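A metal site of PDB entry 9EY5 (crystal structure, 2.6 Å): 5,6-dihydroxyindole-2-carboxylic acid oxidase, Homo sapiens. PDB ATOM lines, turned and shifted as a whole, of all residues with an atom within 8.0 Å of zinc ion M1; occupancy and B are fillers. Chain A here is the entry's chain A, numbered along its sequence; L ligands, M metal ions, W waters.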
ATOM      1  N   HIS A 168     -11.317  31.766  19.293  1.00  0.00           N
ATOM      2  CA  HIS A 168     -12.421  30.864  18.950  1.00  0.00           C
ATOM      3  C   HIS A 168     -12.404  29.612  19.820  1.00  0.00           C
ATOM      4  O   HIS A 168     -13.461  29.144  20.276  1.00  0.00           O
ATOM      5  CB  HIS A 168     -12.329  30.531  17.472  1.00  0.00           C
ATOM      6  CG  HIS A 168     -13.514  29.811  16.928  1.00  0.00           C
ATOM      7  ND1 HIS A 168     -13.693  28.448  17.066  1.00  0.00           N
ATOM      8  CD2 HIS A 168     -14.549  30.250  16.162  1.00  0.00           C
ATOM      9  CE1 HIS A 168     -14.799  28.084  16.435  1.00  0.00           C
ATOM     10  NE2 HIS A 168     -15.334  29.158  15.886  1.00  0.00           N
ATOM     11  N   SER A 190     -20.133  31.107  21.615  1.00  0.00           N
ATOM     12  CA  SER A 190     -20.146  31.717  20.296  1.00  0.00           C
ATOM     13  C   SER A 190     -20.958  30.945  19.265  1.00  0.00           C
ATOM     14  O   SER A 190     -20.961  31.349  18.094  1.00  0.00           O
ATOM     15  CB  SER A 190     -18.720  31.893  19.784  1.00  0.00           C
ATOM     16  OG  SER A 190     -17.941  30.732  20.042  1.00  0.00           O
ATOM     17  N   HIS A 191     -21.636  29.862  19.648  1.00  0.00           N
ATOM     18  CA  HIS A 191     -22.530  29.126  18.770  1.00  0.00           C
ATOM     19  C   HIS A 191     -23.745  28.700  19.557  1.00  0.00           C
ATOM     20  O   HIS A 191     -23.762  28.763  20.793  1.00  0.00           O
ATOM     21  CB  HIS A 191     -21.866  27.893  18.171  1.00  0.00           C
ATOM     22  CG  HIS A 191     -20.447  28.135  17.768  1.00  0.00           C
ATOM     23  ND1 HIS A 191     -19.417  28.199  18.674  1.00  0.00           N
ATOM     24  CD2 HIS A 191     -19.908  28.397  16.555  1.00  0.00           C
ATOM     25  CE1 HIS A 191     -18.293  28.459  18.037  1.00  0.00           C
ATOM     26  NE2 HIS A 191     -18.558  28.570  16.749  1.00  0.00           N
ATOM     27  N   PHE A 196     -24.093  33.976  18.225  1.00  0.00           N
ATOM     28  CA  PHE A 196     -23.289  33.357  17.175  1.00  0.00           C
ATOM     29  C   PHE A 196     -22.921  34.345  16.070  1.00  0.00           C
ATOM     30  O   PHE A 196     -21.744  34.462  15.696  1.00  0.00           O
ATOM     31  CB  PHE A 196     -24.042  32.155  16.576  1.00  0.00           C
ATOM     32  CG  PHE A 196     -23.542  31.744  15.214  1.00  0.00           C
ATOM     33  CD1 PHE A 196     -22.354  31.019  15.086  1.00  0.00           C
ATOM     34  CD2 PHE A 196     -24.243  32.081  14.064  1.00  0.00           C
ATOM     35  CE1 PHE A 196     -21.895  30.642  13.829  1.00  0.00           C
ATOM     36  CE2 PHE A 196     -23.784  31.695  12.803  1.00  0.00           C
ATOM     37  CZ  PHE A 196     -22.603  30.985  12.690  1.00  0.00           C
ATOM     38  N   HIS A 200     -18.982  36.158  15.747  1.00  0.00           N
ATOM     39  CA  HIS A 200     -18.165  35.921  14.569  1.00  0.00           C
ATOM     40  C   HIS A 200     -17.969  37.183  13.741  1.00  0.00           C
ATOM     41  O   HIS A 200     -16.905  37.358  13.128  1.00  0.00           O
ATOM     42  CB  HIS A 200     -18.799  34.827  13.720  1.00  0.00           C
ATOM     43  CG  HIS A 200     -18.636  33.466  14.294  1.00  0.00           C
ATOM     44  ND1 HIS A 200     -19.533  32.911  15.188  1.00  0.00           N
ATOM     45  CD2 HIS A 200     -17.676  32.530  14.086  1.00  0.00           C
ATOM     46  CE1 HIS A 200     -19.125  31.696  15.506  1.00  0.00           C
ATOM     47  NE2 HIS A 200     -17.999  31.446  14.858  1.00  0.00           N
ATOM     48  N   GLU A 336     -27.156  29.877  10.932  1.00  0.00           N
ATOM     49  CA  GLU A 336     -26.159  29.041  11.586  1.00  0.00           C
ATOM     50  C   GLU A 336     -26.216  27.606  11.049  1.00  0.00           C
ATOM     51  O   GLU A 336     -25.181  26.974  10.834  1.00  0.00           O
ATOM     52  CB  GLU A 336     -26.346  29.056  13.105  1.00  0.00           C
ATOM     53  CG  GLU A 336     -25.223  28.316  13.852  1.00  0.00           C
ATOM     54  CD  GLU A 336     -25.280  28.498  15.362  1.00  0.00           C
ATOM     55  OE1 GLU A 336     -26.266  29.092  15.849  1.00  0.00           O
ATOM     56  OE2 GLU A 336     -24.345  28.058  16.070  1.00  0.00           O
ATOM     57  N   HIS A 353     -24.413  27.599   7.086  1.00  0.00           N
ATOM     58  CA  HIS A 353     -23.094  27.732   7.720  1.00  0.00           C
ATOM     59  C   HIS A 353     -22.614  26.402   8.287  1.00  0.00           C
ATOM     60  O   HIS A 353     -21.432  26.052   8.128  1.00  0.00           O
ATOM     61  CB  HIS A 353     -23.126  28.795   8.830  1.00  0.00           C
ATOM     62  CG  HIS A 353     -22.179  28.530   9.976  1.00  0.00           C
ATOM     63  ND1 HIS A 353     -22.482  27.651  10.999  1.00  0.00           N
ATOM     64  CD2 HIS A 353     -20.951  29.018  10.263  1.00  0.00           C
ATOM     65  CE1 HIS A 353     -21.486  27.614  11.859  1.00  0.00           C
ATOM     66  NE2 HIS A 353     -20.559  28.437  11.445  1.00  0.00           N
ATOM     67  N   ASN A 354     -23.488  25.652   8.962  1.00  0.00           N
ATOM     68  CA  ASN A 354     -23.073  24.352   9.505  1.00  0.00           C
ATOM     69  C   ASN A 354     -22.783  23.370   8.394  1.00  0.00           C
ATOM     70  O   ASN A 354     -21.802  22.619   8.461  1.00  0.00           O
ATOM     71  CB  ASN A 354     -24.145  23.769  10.433  1.00  0.00           C
ATOM     72  CG  ASN A 354     -24.136  24.400  11.808  1.00  0.00           C
ATOM     73  OD1 ASN A 354     -23.118  24.953  12.249  1.00  0.00           O
ATOM     74  ND2 ASN A 354     -25.272  24.326  12.493  1.00  0.00           N
ATOM     75  N   ALA A 356     -21.675  24.099   5.432  1.00  0.00           N
ATOM     76  CA  ALA A 356     -20.428  24.463   4.756  1.00  0.00           C
ATOM     77  C   ALA A 356     -19.219  23.939   5.529  1.00  0.00           C
ATOM     78  O   ALA A 356     -18.262  23.454   4.926  1.00  0.00           O
ATOM     79  CB  ALA A 356     -20.340  25.980   4.573  1.00  0.00           C
ATOM     80  N   HIS A 357     -19.270  23.997   6.863  1.00  0.00           N
ATOM     81  CA  HIS A 357     -18.194  23.428   7.662  1.00  0.00           C
ATOM     82  C   HIS A 357     -18.044  21.922   7.439  1.00  0.00           C
ATOM     83  O   HIS A 357     -16.950  21.423   7.188  1.00  0.00           O
ATOM     84  CB  HIS A 357     -18.453  23.695   9.135  1.00  0.00           C
ATOM     85  CG  HIS A 357     -17.969  25.012   9.612  1.00  0.00           C
ATOM     86  ND1 HIS A 357     -16.697  25.198  10.132  1.00  0.00           N
ATOM     87  CD2 HIS A 357     -18.586  26.203   9.709  1.00  0.00           C
ATOM     88  CE1 HIS A 357     -16.560  26.453  10.499  1.00  0.00           C
ATOM     89  NE2 HIS A 357     -17.683  27.091  10.243  1.00  0.00           N
ATOM     90  N   GLY A 364     -11.436  21.862   9.219  1.00  0.00           N
ATOM     91  CA  GLY A 364     -12.428  22.920   9.103  1.00  0.00           C
ATOM     92  C   GLY A 364     -13.785  22.605   9.703  1.00  0.00           C
ATOM     93  O   GLY A 364     -14.684  23.444   9.637  1.00  0.00           O
ATOM     94  N   THR A 367     -15.202  21.832  15.930  1.00  0.00           N
ATOM     95  CA  THR A 367     -15.580  23.150  16.437  1.00  0.00           C
ATOM     96  C   THR A 367     -14.432  23.821  17.191  1.00  0.00           C
ATOM     97  O   THR A 367     -14.296  25.052  17.118  1.00  0.00           O
ATOM     98  CB  THR A 367     -16.824  23.057  17.330  1.00  0.00           C
ATOM     99  OG1 THR A 367     -17.896  22.442  16.603  1.00  0.00           O
ATOM    100  CG2 THR A 367     -17.256  24.499  17.818  1.00  0.00           C
ATOM    101  N   SER A 370     -11.649  24.639  13.963  1.00  0.00           N
ATOM    102  CA  SER A 370     -11.988  25.016  12.589  1.00  0.00           C
ATOM    103  C   SER A 370     -11.269  26.248  12.042  1.00  0.00           C
ATOM    104  O   SER A 370     -10.883  26.214  10.865  1.00  0.00           O
ATOM    105  CB  SER A 370     -13.511  25.187  12.464  1.00  0.00           C
ATOM    106  OG  SER A 370     -14.018  25.870  13.589  1.00  0.00           O
ATOM    107  N   PRO A 371     -11.047  27.336  12.797  1.00  0.00           N
ATOM    108  CA  PRO A 371     -10.333  28.492  12.198  1.00  0.00           C
ATOM    109  C   PRO A 371      -8.918  28.176  11.712  1.00  0.00           C
ATOM    110  O   PRO A 371      -8.331  29.030  11.025  1.00  0.00           O
ATOM    111  CB  PRO A 371     -10.313  29.526  13.333  1.00  0.00           C
ATOM    112  CG  PRO A 371     -11.347  29.094  14.287  1.00  0.00           C
ATOM    113  CD  PRO A 371     -11.436  27.619  14.190  1.00  0.00           C
ATOM    114  N   PHE A 376     -12.033  29.069   6.821  1.00  0.00           N
ATOM    115  CA  PHE A 376     -12.869  29.588   7.903  1.00  0.00           C
ATOM    116  C   PHE A 376     -13.162  31.066   7.689  1.00  0.00           C
ATOM    117  O   PHE A 376     -14.314  31.506   7.752  1.00  0.00           O
ATOM    118  CB  PHE A 376     -12.181  29.379   9.253  1.00  0.00           C
ATOM    119  CG  PHE A 376     -13.018  29.794  10.439  1.00  0.00           C
ATOM    120  CD1 PHE A 376     -13.196  31.135  10.759  1.00  0.00           C
ATOM    121  CD2 PHE A 376     -13.649  28.835  11.231  1.00  0.00           C
ATOM    122  CE1 PHE A 376     -13.992  31.526  11.844  1.00  0.00           C
ATOM    123  CE2 PHE A 376     -14.444  29.211  12.325  1.00  0.00           C
ATOM    124  CZ  PHE A 376     -14.608  30.557  12.632  1.00  0.00           C
ATOM    125  N   LEU A 379     -15.639  31.442   4.639  1.00  0.00           N
ATOM    126  CA  LEU A 379     -16.930  30.947   5.069  1.00  0.00           C
ATOM    127  C   LEU A 379     -17.644  31.971   5.961  1.00  0.00           C
ATOM    128  O   LEU A 379     -18.871  32.171   5.837  1.00  0.00           O
ATOM    129  CB  LEU A 379     -16.716  29.638   5.820  1.00  0.00           C
ATOM    130  CG  LEU A 379     -17.845  28.686   6.140  1.00  0.00           C
ATOM    131  CD1 LEU A 379     -17.179  27.375   6.503  1.00  0.00           C
ATOM    132  CD2 LEU A 379     -18.714  29.177   7.295  1.00  0.00           C
ATOM    133  N   HIS A 380     -16.911  32.647   6.844  1.00  0.00           N
ATOM    134  CA  HIS A 380     -17.591  33.510   7.794  1.00  0.00           C
ATOM    135  C   HIS A 380     -17.831  34.907   7.290  1.00  0.00           C
ATOM    136  O   HIS A 380     -18.847  35.511   7.661  1.00  0.00           O
ATOM    137  CB  HIS A 380     -16.834  33.551   9.109  1.00  0.00           C
ATOM    138  CG  HIS A 380     -17.239  32.420   9.971  1.00  0.00           C
ATOM    139  ND1 HIS A 380     -18.405  32.446  10.725  1.00  0.00           N
ATOM    140  CD2 HIS A 380     -16.757  31.164  10.067  1.00  0.00           C
ATOM    141  CE1 HIS A 380     -18.560  31.278  11.308  1.00  0.00           C
ATOM    142  NE2 HIS A 380     -17.573  30.496  10.923  1.00  0.00           N
ATOM    143  N   THR A 383     -21.086  34.257   5.700  1.00  0.00           N
ATOM    144  CA  THR A 383     -22.138  34.217   6.720  1.00  0.00           C
ATOM    145  C   THR A 383     -22.463  35.627   7.185  1.00  0.00           C
ATOM    146  O   THR A 383     -23.634  36.008   7.264  1.00  0.00           O
ATOM    147  CB  THR A 383     -21.709  33.364   7.917  1.00  0.00           C
ATOM    148  OG1 THR A 383     -21.302  32.079   7.467  1.00  0.00           O
ATOM    149  CG2 THR A 383     -22.863  33.187   8.896  1.00  0.00           C
HETATM  150  O1  LIG L   1     -18.543  21.554  12.214  1.00  0.00           O
HETATM  151  N1  LIG L   1     -22.934  20.751  13.451  1.00  0.00           N
HETATM  152  C1  LIG L   1     -21.519  21.165  13.409  1.00  0.00           C
HETATM  153  C2  LIG L   1     -20.970  21.350  14.838  1.00  0.00           C
HETATM  154  O2  LIG L   1     -19.830  20.888  15.138  1.00  0.00           O
HETATM  155  C3  LIG L   1     -21.340  22.489  12.560  1.00  0.00           C
HETATM  156  C4  LIG L   1     -20.092  23.343  12.955  1.00  0.00           C
HETATM  157  C5  LIG L   1     -18.793  22.865  12.774  1.00  0.00           C
HETATM  158  C6  LIG L   1     -20.243  24.662  13.501  1.00  0.00           C
HETATM  159  C7  LIG L   1     -17.643  23.654  13.134  1.00  0.00           C
HETATM  160  C8  LIG L   1     -19.128  25.461  13.889  1.00  0.00           C
HETATM  161  C9  LIG L   1     -17.828  24.937  13.690  1.00  0.00           C
HETATM  162  O3  LIG L   1     -16.642  25.706  14.048  1.00  0.00           O
HETATM  163  O4  LIG L   1     -21.650  21.967  15.732  1.00  0.00           O
HETATM  164 ZN    ZN M   1     -18.386  28.615  11.733  1.00  0.00          ZN
HETATM  165 ZN    ZN M   2     -17.376  29.372  15.030  1.00  0.00          ZN
HETATM  166  O   HOH W   1     -17.546  28.243  13.349  1.00  0.00           O
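The side-chain hydroxyl (OG) of Ser 370 lies within hydrogen-bond range of an oxygen (O3) of the ligand (2.7 Å). OG1 of Thr 367 is in hydrogen-bond range of O2 of the ligand, at 2.9 Å.
A ring nitrogen (ND1) of His 353 sits at hydrogen-bond distance from the side-chain amide oxygen (OD1) of Asn 354 (3.0 Å). A ring nitrogen (ND1) of His 353 sits at hydrogen-bond distance from the backbone carbonyl oxygen (O) of Glu 336, 2.8 Å away. O of Gly 364 lies within hydrogen-bond range of ND1 of His 357, at 2.7 Å.
Water W1 is bound to zinc ion M1 (1.9 Å). Zinc ion M1 is bound by a ring nitrogen (NE2) of His 353. Zinc ion M1 is bound by NE2 of His 380 (2.2 Å). NE2 of His 357 is bound to zinc ion M1 (2.2 Å).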
